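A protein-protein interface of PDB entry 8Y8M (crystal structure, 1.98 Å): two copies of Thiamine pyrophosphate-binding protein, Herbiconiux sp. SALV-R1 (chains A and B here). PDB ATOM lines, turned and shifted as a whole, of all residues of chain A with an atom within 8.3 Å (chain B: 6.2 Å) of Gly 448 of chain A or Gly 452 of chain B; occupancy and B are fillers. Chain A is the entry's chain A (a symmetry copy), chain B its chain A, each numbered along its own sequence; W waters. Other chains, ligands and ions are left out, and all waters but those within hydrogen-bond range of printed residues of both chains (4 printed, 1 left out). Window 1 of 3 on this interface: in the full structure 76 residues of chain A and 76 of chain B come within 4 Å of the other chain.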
ATOM      1  N   MET A  50     -36.273  -1.721 -29.437  1.00  0.00           N
ATOM      2  CA  MET A  50     -36.791  -0.452 -28.968  1.00  0.00           C
ATOM      3  C   MET A  50     -37.221   0.405 -30.140  1.00  0.00           C
ATOM      4  O   MET A  50     -38.246   1.105 -30.078  1.00  0.00           O
ATOM      5  CB  MET A  50     -35.757   0.239 -28.051  1.00  0.00           C
ATOM      6  CG  MET A  50     -35.922   1.739 -27.893  1.00  0.00           C
ATOM      7  SD  MET A  50     -34.497   2.606 -27.090  1.00  0.00           S
ATOM      8  CE  MET A  50     -33.538   3.247 -28.518  1.00  0.00           C
ATOM      9  N   ASP A 390     -36.540  15.606 -31.313  1.00  0.00           N
ATOM     10  CA  ASP A 390     -36.013  14.896 -30.150  1.00  0.00           C
ATOM     11  C   ASP A 390     -35.013  15.821 -29.468  1.00  0.00           C
ATOM     12  O   ASP A 390     -34.766  16.940 -29.928  1.00  0.00           O
ATOM     13  CB  ASP A 390     -35.379  13.559 -30.569  1.00  0.00           C
ATOM     14  CG  ASP A 390     -35.250  12.518 -29.374  1.00  0.00           C
ATOM     15  OD1 ASP A 390     -35.534  12.843 -28.207  1.00  0.00           O
ATOM     16  OD2 ASP A 390     -34.882  11.344 -29.624  1.00  0.00           O
ATOM     17  N   MET A 419     -36.138  11.112 -24.024  1.00  0.00           N
ATOM     18  CA  MET A 419     -35.016  11.435 -24.911  1.00  0.00           C
ATOM     19  C   MET A 419     -34.570  10.165 -25.598  1.00  0.00           C
ATOM     20  O   MET A 419     -34.396   9.148 -24.936  1.00  0.00           O
ATOM     21  CB  MET A 419     -33.838  12.006 -24.124  1.00  0.00           C
ATOM     22  CG  MET A 419     -34.144  13.304 -23.407  1.00  0.00           C
ATOM     23  SD  MET A 419     -34.706  14.587 -24.565  1.00  0.00           S
ATOM     24  CE  MET A 419     -36.468  14.621 -24.188  1.00  0.00           C
ATOM     25  N   GLY A 420     -34.442  10.190 -26.931  1.00  0.00           N
ATOM     26  CA  GLY A 420     -33.923   9.034 -27.632  1.00  0.00           C
ATOM     27  C   GLY A 420     -34.887   8.366 -28.595  1.00  0.00           C
ATOM     28  O   GLY A 420     -34.426   7.599 -29.463  1.00  0.00           O
ATOM     29  N   VAL A 423     -34.984   8.681 -33.475  1.00  0.00           N
ATOM     30  CA  VAL A 423     -34.420   8.020 -34.641  1.00  0.00           C
ATOM     31  C   VAL A 423     -35.333   6.893 -35.108  1.00  0.00           C
ATOM     32  O   VAL A 423     -35.619   6.758 -36.314  1.00  0.00           O
ATOM     33  CB  VAL A 423     -32.957   7.567 -34.364  1.00  0.00           C
ATOM     34  CG1 VAL A 423     -32.387   6.651 -35.472  1.00  0.00           C
ATOM     35  CG2 VAL A 423     -32.036   8.806 -34.264  1.00  0.00           C
ATOM     36  N   THR A 442     -32.640  16.532 -33.767  1.00  0.00           N
ATOM     37  CA  THR A 442     -32.438  15.851 -32.496  1.00  0.00           C
ATOM     38  C   THR A 442     -31.171  16.427 -31.866  1.00  0.00           C
ATOM     39  O   THR A 442     -30.363  17.075 -32.547  1.00  0.00           O
ATOM     40  CB  THR A 442     -32.337  14.347 -32.702  1.00  0.00           C
ATOM     41  OG1 THR A 442     -32.178  13.740 -31.434  1.00  0.00           O
ATOM     42  CG2 THR A 442     -31.036  14.008 -33.559  1.00  0.00           C
ATOM     43  N   GLY A 443     -31.028  16.259 -30.546  1.00  0.00           N
ATOM     44  CA  GLY A 443     -29.827  16.727 -29.879  1.00  0.00           C
ATOM     45  C   GLY A 443     -28.742  15.671 -29.898  1.00  0.00           C
ATOM     46  O   GLY A 443     -28.981  14.550 -30.352  1.00  0.00           O
ATOM     47  N   ASP A 444     -27.525  16.051 -29.440  1.00  0.00           N
ATOM     48  CA  ASP A 444     -26.429  15.087 -29.484  1.00  0.00           C
ATOM     49  C   ASP A 444     -26.630  14.006 -28.427  1.00  0.00           C
ATOM     50  O   ASP A 444     -26.201  12.870 -28.637  1.00  0.00           O
ATOM     51  CB  ASP A 444     -25.064  15.751 -29.248  1.00  0.00           C
ATOM     52  CG  ASP A 444     -25.083  16.743 -28.104  1.00  0.00           C
ATOM     53  OD1 ASP A 444     -26.009  17.607 -27.997  1.00  0.00           O
ATOM     54  OD2 ASP A 444     -24.128  16.672 -27.302  1.00  0.00           O
ATOM     55  N   GLY A 445     -27.251  14.352 -27.292  1.00  0.00           N
ATOM     56  CA  GLY A 445     -27.594  13.357 -26.283  1.00  0.00           C
ATOM     57  C   GLY A 445     -28.569  12.318 -26.819  1.00  0.00           C
ATOM     58  O   GLY A 445     -28.272  11.115 -26.819  1.00  0.00           O
ATOM     59  N   ALA A 446     -29.726  12.774 -27.323  1.00  0.00           N
ATOM     60  CA  ALA A 446     -30.766  11.831 -27.734  1.00  0.00           C
ATOM     61  C   ALA A 446     -30.276  10.920 -28.843  1.00  0.00           C
ATOM     62  O   ALA A 446     -30.625   9.733 -28.894  1.00  0.00           O
ATOM     63  CB  ALA A 446     -32.011  12.597 -28.195  1.00  0.00           C
ATOM     64  N   VAL A 447     -29.515  11.472 -29.793  1.00  0.00           N
ATOM     65  CA  VAL A 447     -29.167  10.660 -30.953  1.00  0.00           C
ATOM     66  C   VAL A 447     -28.292   9.475 -30.558  1.00  0.00           C
ATOM     67  O   VAL A 447     -28.323   8.427 -31.222  1.00  0.00           O
ATOM     68  CB  VAL A 447     -28.500  11.535 -32.046  1.00  0.00           C
ATOM     69  CG1 VAL A 447     -27.029  11.650 -31.769  1.00  0.00           C
ATOM     70  CG2 VAL A 447     -28.722  10.890 -33.414  1.00  0.00           C
ATOM     71  N   GLY A 448     -27.518   9.592 -29.470  1.00  0.00           N
ATOM     72  CA  GLY A 448     -26.650   8.474 -29.113  1.00  0.00           C
ATOM     73  C   GLY A 448     -27.402   7.217 -28.663  1.00  0.00           C
ATOM     74  O   GLY A 448     -26.783   6.150 -28.604  1.00  0.00           O
ATOM     75  N   TYR A 449     -28.728   7.303 -28.381  1.00  0.00           N
ATOM     76  CA  TYR A 449     -29.493   6.071 -28.082  1.00  0.00           C
ATOM     77  C   TYR A 449     -29.496   5.059 -29.220  1.00  0.00           C
ATOM     78  O   TYR A 449     -29.623   3.848 -28.968  1.00  0.00           O
ATOM     79  CB  TYR A 449     -30.948   6.382 -27.725  1.00  0.00           C
ATOM     80  CG  TYR A 449     -31.169   6.886 -26.307  1.00  0.00           C
ATOM     81  CD1 TYR A 449     -30.864   8.188 -25.938  1.00  0.00           C
ATOM     82  CD2 TYR A 449     -31.647   6.016 -25.334  1.00  0.00           C
ATOM     83  CE1 TYR A 449     -31.003   8.628 -24.647  1.00  0.00           C
ATOM     84  CE2 TYR A 449     -31.821   6.466 -24.009  1.00  0.00           C
ATOM     85  CZ  TYR A 449     -31.483   7.769 -23.689  1.00  0.00           C
ATOM     86  OH  TYR A 449     -31.633   8.212 -22.397  1.00  0.00           O
ATOM     87  N   SER A 450     -29.474   5.538 -30.488  1.00  0.00           N
ATOM     88  CA  SER A 450     -29.951   4.763 -31.650  1.00  0.00           C
ATOM     89  C   SER A 450     -29.010   4.882 -32.849  1.00  0.00           C
ATOM     90  O   SER A 450     -29.447   4.789 -34.027  1.00  0.00           O
ATOM     91  CB  SER A 450     -31.331   5.255 -32.034  1.00  0.00           C
ATOM     92  OG  SER A 450     -32.226   5.019 -30.934  1.00  0.00           O
ATOM     93  N   LEU A 451     -27.714   5.073 -32.579  1.00  0.00           N
ATOM     94  CA  LEU A 451     -26.756   5.273 -33.678  1.00  0.00           C
ATOM     95  C   LEU A 451     -26.811   4.119 -34.687  1.00  0.00           C
ATOM     96  O   LEU A 451     -26.702   4.336 -35.904  1.00  0.00           O
ATOM     97  CB  LEU A 451     -25.357   5.396 -33.094  1.00  0.00           C
ATOM     98  CG  LEU A 451     -25.183   6.667 -32.252  1.00  0.00           C
ATOM     99  CD1 LEU A 451     -23.783   6.595 -31.570  1.00  0.00           C
ATOM    100  CD2 LEU A 451     -25.348   7.889 -33.123  1.00  0.00           C
ATOM    101  N   GLY A 452     -26.951   2.881 -34.192  1.00  0.00           N
ATOM    102  CA  GLY A 452     -27.013   1.699 -35.043  1.00  0.00           C
ATOM    103  C   GLY A 452     -28.099   1.738 -36.101  1.00  0.00           C
ATOM    104  O   GLY A 452     -27.985   1.013 -37.091  1.00  0.00           O
ATOM    105  N   PHE A 454     -28.719   4.015 -38.187  1.00  0.00           N
ATOM    106  CA  PHE A 454     -28.231   4.487 -39.490  1.00  0.00           C
ATOM    107  C   PHE A 454     -28.052   3.295 -40.409  1.00  0.00           C
ATOM    108  O   PHE A 454     -28.388   3.348 -41.602  1.00  0.00           O
ATOM    109  CB  PHE A 454     -26.917   5.277 -39.351  1.00  0.00           C
ATOM    110  CG  PHE A 454     -27.108   6.695 -38.895  1.00  0.00           C
ATOM    111  CD1 PHE A 454     -27.777   7.615 -39.685  1.00  0.00           C
ATOM    112  CD2 PHE A 454     -26.657   7.085 -37.636  1.00  0.00           C
ATOM    113  CE1 PHE A 454     -27.949   8.916 -39.269  1.00  0.00           C
ATOM    114  CE2 PHE A 454     -26.835   8.386 -37.174  1.00  0.00           C
ATOM    115  CZ  PHE A 454     -27.490   9.311 -38.006  1.00  0.00           C
ATOM    116  N   VAL A 468     -28.412  16.720 -36.310  1.00  0.00           N
ATOM    117  CA  VAL A 468     -28.029  16.735 -34.900  1.00  0.00           C
ATOM    118  C   VAL A 468     -27.627  18.138 -34.483  1.00  0.00           C
ATOM    119  O   VAL A 468     -26.631  18.682 -34.959  1.00  0.00           O
ATOM    120  CB  VAL A 468     -26.880  15.757 -34.632  1.00  0.00           C
ATOM    121  CG1 VAL A 468     -26.581  15.683 -33.097  1.00  0.00           C
ATOM    122  CG2 VAL A 468     -27.224  14.383 -35.254  1.00  0.00           C
ATOM    123  N   TRP A 474     -25.763  16.935 -22.514  1.00  0.00           N
ATOM    124  CA  TRP A 474     -27.166  16.701 -22.217  1.00  0.00           C
ATOM    125  C   TRP A 474     -27.710  18.052 -21.810  1.00  0.00           C
ATOM    126  O   TRP A 474     -27.611  18.440 -20.643  1.00  0.00           O
ATOM    127  CB  TRP A 474     -27.358  15.721 -21.080  1.00  0.00           C
ATOM    128  CG  TRP A 474     -26.887  14.357 -21.250  1.00  0.00           C
ATOM    129  CD1 TRP A 474     -25.740  13.814 -20.703  1.00  0.00           C
ATOM    130  CD2 TRP A 474     -27.467  13.330 -22.066  1.00  0.00           C
ATOM    131  NE1 TRP A 474     -25.634  12.487 -21.060  1.00  0.00           N
ATOM    132  CE2 TRP A 474     -26.672  12.160 -21.893  1.00  0.00           C
ATOM    133  CE3 TRP A 474     -28.610  13.260 -22.871  1.00  0.00           C
ATOM    134  CZ2 TRP A 474     -26.977  10.951 -22.502  1.00  0.00           C
ATOM    135  CZ3 TRP A 474     -28.910  12.051 -23.491  1.00  0.00           C
ATOM    136  CH2 TRP A 474     -28.092  10.914 -23.306  1.00  0.00           C
ATOM    137  N   LEU A 495     -20.984  16.459 -22.680  1.00  0.00           N
ATOM    138  CA  LEU A 495     -20.737  15.418 -23.675  1.00  0.00           C
ATOM    139  C   LEU A 495     -19.723  15.925 -24.706  1.00  0.00           C
ATOM    140  O   LEU A 495     -20.069  16.100 -25.887  1.00  0.00           O
ATOM    141  CB  LEU A 495     -22.029  14.935 -24.371  1.00  0.00           C
ATOM    142  CG  LEU A 495     -23.113  14.244 -23.534  1.00  0.00           C
ATOM    143  CD1 LEU A 495     -24.389  14.067 -24.391  1.00  0.00           C
ATOM    144  CD2 LEU A 495     -22.567  12.889 -23.011  1.00  0.00           C
ATOM    145  N   ASN A 497     -17.211  14.914 -26.622  1.00  0.00           N
ATOM    146  CA  ASN A 497     -16.496  13.836 -27.283  1.00  0.00           C
ATOM    147  C   ASN A 497     -17.365  13.290 -28.404  1.00  0.00           C
ATOM    148  O   ASN A 497     -18.599  13.259 -28.293  1.00  0.00           O
ATOM    149  CB  ASN A 497     -16.147  12.739 -26.273  1.00  0.00           C
ATOM    150  CG  ASN A 497     -15.489  11.541 -26.921  1.00  0.00           C
ATOM    151  OD1 ASN A 497     -14.371  11.635 -27.476  1.00  0.00           O
ATOM    152  ND2 ASN A 497     -16.166  10.407 -26.872  1.00  0.00           N
ATOM    153  N   TYR A 500     -20.779  12.511 -34.491  1.00  0.00           N
ATOM    154  CA  TYR A 500     -21.955  11.787 -34.949  1.00  0.00           C
ATOM    155  C   TYR A 500     -21.963  11.667 -36.467  1.00  0.00           C
ATOM    156  O   TYR A 500     -22.388  10.634 -36.996  1.00  0.00           O
ATOM    157  CB  TYR A 500     -23.239  12.494 -34.412  1.00  0.00           C
ATOM    158  CG  TYR A 500     -23.190  12.576 -32.932  1.00  0.00           C
ATOM    159  CD1 TYR A 500     -23.323  11.417 -32.122  1.00  0.00           C
ATOM    160  CD2 TYR A 500     -22.750  13.752 -32.339  1.00  0.00           C
ATOM    161  CE1 TYR A 500     -23.216  11.482 -30.723  1.00  0.00           C
ATOM    162  CE2 TYR A 500     -22.595  13.835 -30.932  1.00  0.00           C
ATOM    163  CZ  TYR A 500     -22.843  12.706 -30.129  1.00  0.00           C
ATOM    164  OH  TYR A 500     -22.652  12.828 -28.749  1.00  0.00           O
ATOM    165  N   VAL A 503     -19.872   8.653 -37.159  1.00  0.00           N
ATOM    166  CA  VAL A 503     -20.590   7.402 -36.883  1.00  0.00           C
ATOM    167  C   VAL A 503     -21.510   7.062 -38.046  1.00  0.00           C
ATOM    168  O   VAL A 503     -21.524   5.942 -38.546  1.00  0.00           O
ATOM    169  CB  VAL A 503     -21.399   7.518 -35.565  1.00  0.00           C
ATOM    170  CG1 VAL A 503     -22.338   6.306 -35.417  1.00  0.00           C
ATOM    171  CG2 VAL A 503     -20.439   7.609 -34.348  1.00  0.00           C
ATOM    172  N   ARG B  47     -25.041   6.206 -22.335  1.00  0.00           N
ATOM    173  CA  ARG B  47     -25.748   6.783 -23.473  1.00  0.00           C
ATOM    174  C   ARG B  47     -27.175   6.222 -23.624  1.00  0.00           C
ATOM    175  O   ARG B  47     -27.929   6.668 -24.494  1.00  0.00           O
ATOM    176  CB  ARG B  47     -24.959   6.540 -24.761  1.00  0.00           C
ATOM    177  CG  ARG B  47     -23.669   7.341 -24.858  1.00  0.00           C
ATOM    178  CD  ARG B  47     -23.831   8.819 -24.543  1.00  0.00           C
ATOM    179  NE  ARG B  47     -24.719   9.487 -25.490  1.00  0.00           N
ATOM    180  CZ  ARG B  47     -24.333  10.438 -26.330  1.00  0.00           C
ATOM    181  NH1 ARG B  47     -23.068  10.836 -26.348  1.00  0.00           N
ATOM    182  NH2 ARG B  47     -25.210  10.991 -27.157  1.00  0.00           N
ATOM    183  N   ASN B  48     -27.572   5.284 -22.758  1.00  0.00           N
ATOM    184  CA  ASN B  48     -28.876   4.622 -22.731  1.00  0.00           C
ATOM    185  C   ASN B  48     -29.065   4.033 -21.347  1.00  0.00           C
ATOM    186  O   ASN B  48     -28.165   3.338 -20.860  1.00  0.00           O
ATOM    187  CB  ASN B  48     -28.948   3.528 -23.804  1.00  0.00           C
ATOM    188  CG  ASN B  48     -30.321   2.948 -23.951  1.00  0.00           C
ATOM    189  OD1 ASN B  48     -31.221   3.168 -23.111  1.00  0.00           O
ATOM    190  ND2 ASN B  48     -30.547   2.308 -25.081  1.00  0.00           N
ATOM    191  N   TYR B 449     -26.653  -2.709 -30.769  1.00  0.00           N
ATOM    192  CA  TYR B 449     -27.561  -2.139 -29.747  1.00  0.00           C
ATOM    193  C   TYR B 449     -27.001  -0.906 -29.050  1.00  0.00           C
ATOM    194  O   TYR B 449     -27.778  -0.054 -28.587  1.00  0.00           O
ATOM    195  CB  TYR B 449     -27.918  -3.167 -28.672  1.00  0.00           C
ATOM    196  CG  TYR B 449     -28.979  -4.178 -29.076  1.00  0.00           C
ATOM    197  CD1 TYR B 449     -28.691  -5.246 -29.915  1.00  0.00           C
ATOM    198  CD2 TYR B 449     -30.288  -4.015 -28.638  1.00  0.00           C
ATOM    199  CE1 TYR B 449     -29.658  -6.123 -30.332  1.00  0.00           C
ATOM    200  CE2 TYR B 449     -31.286  -4.930 -29.038  1.00  0.00           C
ATOM    201  CZ  TYR B 449     -30.948  -5.965 -29.891  1.00  0.00           C
ATOM    202  OH  TYR B 449     -31.917  -6.851 -30.299  1.00  0.00           O
ATOM    203  N   SER B 450     -25.660  -0.846 -28.858  1.00  0.00           N
ATOM    204  CA  SER B 450     -25.032  -0.012 -27.816  1.00  0.00           C
ATOM    205  C   SER B 450     -23.800   0.729 -28.334  1.00  0.00           C
ATOM    206  O   SER B 450     -22.849   1.026 -27.562  1.00  0.00           O
ATOM    207  CB  SER B 450     -24.642  -0.895 -26.649  1.00  0.00           C
ATOM    208  OG  SER B 450     -25.833  -1.485 -26.100  1.00  0.00           O
ATOM    209  N   LEU B 451     -23.795   1.054 -29.632  1.00  0.00           N
ATOM    210  CA  LEU B 451     -22.613   1.700 -30.224  1.00  0.00           C
ATOM    211  C   LEU B 451     -22.237   2.981 -29.468  1.00  0.00           C
ATOM    212  O   LEU B 451     -21.047   3.278 -29.278  1.00  0.00           O
ATOM    213  CB  LEU B 451     -22.905   2.016 -31.683  1.00  0.00           C
ATOM    214  CG  LEU B 451     -23.065   0.749 -32.535  1.00  0.00           C
ATOM    215  CD1 LEU B 451     -23.530   1.192 -33.956  1.00  0.00           C
ATOM    216  CD2 LEU B 451     -21.770  -0.025 -32.558  1.00  0.00           C
ATOM    217  N   GLY B 452     -23.244   3.765 -29.057  1.00  0.00           N
ATOM    218  CA  GLY B 452     -23.021   5.011 -28.332  1.00  0.00           C
ATOM    219  C   GLY B 452     -22.199   4.868 -27.067  1.00  0.00           C
ATOM    220  O   GLY B 452     -21.629   5.863 -26.618  1.00  0.00           O
ATOM    221  N   GLU B 453     -22.184   3.668 -26.427  1.00  0.00           N
ATOM    222  CA  GLU B 453     -21.403   3.495 -25.196  1.00  0.00           C
ATOM    223  C   GLU B 453     -19.883   3.557 -25.443  1.00  0.00           C
ATOM    224  O   GLU B 453     -19.114   3.709 -24.475  1.00  0.00           O
ATOM    225  CB  GLU B 453     -21.722   2.151 -24.525  1.00  0.00           C
ATOM    226  CG  GLU B 453     -23.257   1.959 -24.109  1.00  0.00           C
ATOM    227  CD  GLU B 453     -23.900   3.152 -23.429  1.00  0.00           C
ATOM    228  OE1 GLU B 453     -23.245   3.893 -22.631  1.00  0.00           O
ATOM    229  OE2 GLU B 453     -25.141   3.270 -23.588  1.00  0.00           O
ATOM    230  N   PHE B 454     -19.412   3.448 -26.693  1.00  0.00           N
ATOM    231  CA  PHE B 454     -17.986   3.733 -26.902  1.00  0.00           C
ATOM    232  C   PHE B 454     -17.678   5.118 -26.367  1.00  0.00           C
ATOM    233  O   PHE B 454     -16.638   5.344 -25.732  1.00  0.00           O
ATOM    234  CB  PHE B 454     -17.597   3.618 -28.387  1.00  0.00           C
ATOM    235  CG  PHE B 454     -17.394   2.204 -28.851  1.00  0.00           C
ATOM    236  CD1 PHE B 454     -16.368   1.426 -28.345  1.00  0.00           C
ATOM    237  CD2 PHE B 454     -18.283   1.641 -29.765  1.00  0.00           C
ATOM    238  CE1 PHE B 454     -16.179   0.131 -28.774  1.00  0.00           C
ATOM    239  CE2 PHE B 454     -18.137   0.327 -30.202  1.00  0.00           C
ATOM    240  CZ  PHE B 454     -17.068  -0.434 -29.697  1.00  0.00           C
ATOM    241  N   ASP B 455     -18.610   6.051 -26.543  1.00  0.00           N
ATOM    242  CA  ASP B 455     -18.348   7.396 -26.025  1.00  0.00           C
ATOM    243  C   ASP B 455     -18.323   7.391 -24.493  1.00  0.00           C
ATOM    244  O   ASP B 455     -17.511   8.095 -23.872  1.00  0.00           O
ATOM    245  CB  ASP B 455     -19.402   8.364 -26.529  1.00  0.00           C
ATOM    246  CG  ASP B 455     -19.488   9.603 -25.683  1.00  0.00           C
ATOM    247  OD1 ASP B 455     -18.571  10.404 -25.765  1.00  0.00           O
ATOM    248  OD2 ASP B 455     -20.508   9.857 -25.009  1.00  0.00           O
ATOM    249  N   SER B 456     -19.210   6.586 -23.879  1.00  0.00           N
ATOM    250  CA  SER B 456     -19.279   6.468 -22.415  1.00  0.00           C
ATOM    251  C   SER B 456     -17.969   5.933 -21.848  1.00  0.00           C
ATOM    252  O   SER B 456     -17.454   6.459 -20.846  1.00  0.00           O
ATOM    253  CB  SER B 456     -20.428   5.516 -22.018  1.00  0.00           C
ATOM    254  OG  SER B 456     -21.685   6.003 -22.478  1.00  0.00           O
ATOM    255  N   MET B 457     -17.423   4.875 -22.475  1.00  0.00           N
ATOM    256  CA  MET B 457     -16.117   4.352 -22.058  1.00  0.00           C
ATOM    257  C   MET B 457     -15.027   5.406 -22.147  1.00  0.00           C
ATOM    258  O   MET B 457     -14.212   5.534 -21.210  1.00  0.00           O
ATOM    259  CB  MET B 457     -15.693   3.116 -22.869  1.00  0.00           C
ATOM    260  CG  MET B 457     -16.732   1.996 -22.911  1.00  0.00           C
ATOM    261  SD  MET B 457     -16.357   0.858 -24.287  1.00  0.00           S
ATOM    262  CE  MET B 457     -17.679  -0.307 -23.809  1.00  0.00           C
ATOM    263  N   VAL B 503     -17.175   3.196 -36.480  1.00  0.00           N
ATOM    264  CA  VAL B 503     -18.064   3.811 -35.485  1.00  0.00           C
ATOM    265  C   VAL B 503     -17.296   4.091 -34.202  1.00  0.00           C
ATOM    266  O   VAL B 503     -17.353   5.183 -33.647  1.00  0.00           O
ATOM    267  CB  VAL B 503     -19.282   2.893 -35.202  1.00  0.00           C
ATOM    268  CG1 VAL B 503     -20.067   3.423 -33.988  1.00  0.00           C
ATOM    269  CG2 VAL B 503     -20.203   2.817 -36.450  1.00  0.00           C
ATOM    270  N   LEU B 507     -16.183   7.809 -32.202  1.00  0.00           N
ATOM    271  CA  LEU B 507     -16.591   8.072 -30.824  1.00  0.00           C
ATOM    272  C   LEU B 507     -15.387   8.178 -29.889  1.00  0.00           C
ATOM    273  O   LEU B 507     -15.555   8.137 -28.660  1.00  0.00           O
ATOM    274  CB  LEU B 507     -17.521   6.940 -30.405  1.00  0.00           C
ATOM    275  CG  LEU B 507     -18.890   6.945 -31.125  1.00  0.00           C
ATOM    276  CD1 LEU B 507     -19.908   6.061 -30.515  1.00  0.00           C
ATOM    277  CD2 LEU B 507     -19.448   8.369 -30.890  1.00  0.00           C
HETATM  278  O   HOH W   1     -27.299   8.842 -25.895  1.00  0.00           O
HETATM  279  O   HOH W   2     -28.337   2.227 -26.891  1.00  0.00           O
HETATM  280  O   HOH W   3     -26.131   3.787 -29.698  1.00  0.00           O
HETATM  281  O   HOH W   4     -30.183   1.125 -29.780  1.00  0.00           O
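CA of Gly 448 of chain A touches NH2 of Arg 47 of chain B, 3.5 Å away.
CA of Gly 452 of chain B touches O of Gly 448 of chain A (3.9 Å).
Tyr 449 of chain A touches Arg 47 of chain B.
CE2 of Tyr 449 of chain A touches OD1 of Asn 48 of chain B, at 3.5 Å.
Leu 451 of chain A touches Gly 452 of chain B (CD1 to CA, 3.7 Å).
Gly 452 of chain A touches Leu 451 of chain B.
CD2 of Leu 495 of chain A touches NH1 of Arg 47 of chain B (3.9 Å).
CG1 of Val 503 of chain A touches CG1 of Val 503 of chain B, at 3.9 Å.
Val 503 of chain A touches Leu 507 of chain B.
Of chain B, only Arg 47 and Gly 452 come within 4 Å of Gly 448 of chain A.
Printed residues of chain B within 4 Å of Tyr 449 of chain A: Arg 47 (3.6 Å) and Asn 48 (3.5 Å).
Of the printed residues of chain A, Asn 48 of chain B touches Tyr 449 (3.5 Å).
Of the printed residues of chain A, Val 503 of chain B touches Val 503.
Of the printed residues of chain A, Leu 451 of chain B touches Gly 452 (3.7 Å).
Met 457 of chain B touches none of the printed residues of chain A.
The nearest residue of chain B that does not touch Gly 448 of chain A is Leu 451 of chain B (5.6 Å).
The nearest residue of chain A that does not touch Gly 452 of chain B is Tyr 449 of chain A (6.2 Å).
Hydrophobic or aromatic side chains of chain A that line the printed part of chain B: Tyr 449, Leu 451, Leu 495, Tyr 500 and Val 503.
Printed residues of chain B that touch a printed residue of chain A: Arg 47, Asn 48, Leu 451, Gly 452, Asp 455, Val 503 and Leu 507.
Along chain B the printed residues that touch a printed residue of chain A span positions 47 to 507.
Among the printed residues, 14 pairs touch across the chains.
Among the printed residues, no Asp or Glu carboxylate lies within 4 Å of a Lys or Arg side-chain nitrogen of the other chain.
The guanidinium group of Arg 47 of chain B is in hydrogen-bond range of the backbone carbonyl oxygen of Asp 444 of chain A (2.6 Å).
The side-chain amide nitrogen (ND2) of Asn 497 of chain A sits at hydrogen-bond distance from the backbone carbonyl oxygen (O) of Leu 507 of chain B.
The side-chain carboxylate of Asp 455 of chain B is in hydrogen-bond range of the side-chain amide nitrogen of Asn 497 of chain A, at 2.6 Å.
NH1 of Arg 47 of chain B lies within hydrogen-bond range of OH of Tyr 500 of chain A (3.1 Å).
The backbone carbonyl oxygen (O) of Gly 445 of chain A is in hydrogen-bond range of the guanidinium group (NH2) of Arg 47 of chain B, 3.1 Å away.
Leu 451 of chain A touches Gly 452 of chain B, and with the chains exchanged Gly 452 of chain A touches Leu 451 of chain B.
Val 503 of chain A touches its own counterpart, Val 503 of chain B.
6 positions are printed for both chains.
Of the 14 pairs that touch across the chains among the printed residues, 3 have their exchanged pair printed and touching as well.
N of Arg 47 of chain B lies within hydrogen-bond range of OG of Ser 456 of chain B (3.4 Å).
The backbone NH (N) of Arg 47 of chain B sits at hydrogen-bond distance from the side-chain carboxylate (OE1) of Glu 453 of chain B, at 2.9 Å.
The guanidinium group of Arg 47 of chain B lies within salt-bridge range of the side-chain carboxylate of Asp 455 of chain B (3.1 Å).
The backbone NH of Asn 48 of chain B lies within hydrogen-bond range of the side-chain carboxylate of Glu 453 of chain B, at 3.3 Å.
Water W1 lies within hydrogen-bond range of O of Gly 445 of chain A (2.6 Å), O of Arg 47 of chain B (2.7 Å) and N of Tyr 449 of chain A (3.3 Å).
Water W3 bridges O of Gly 448 of chain A (2.7 Å) and N of Gly 452 of chain B (3.0 Å).
Water W2 lies within hydrogen-bond range of ND2 of Asn 48 of chain B, O of Tyr 449 of chain B and O of Tyr 449 of chain A.
Water W4 bridges O of Tyr 449 of chain A and O of Tyr 449 of chain B.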
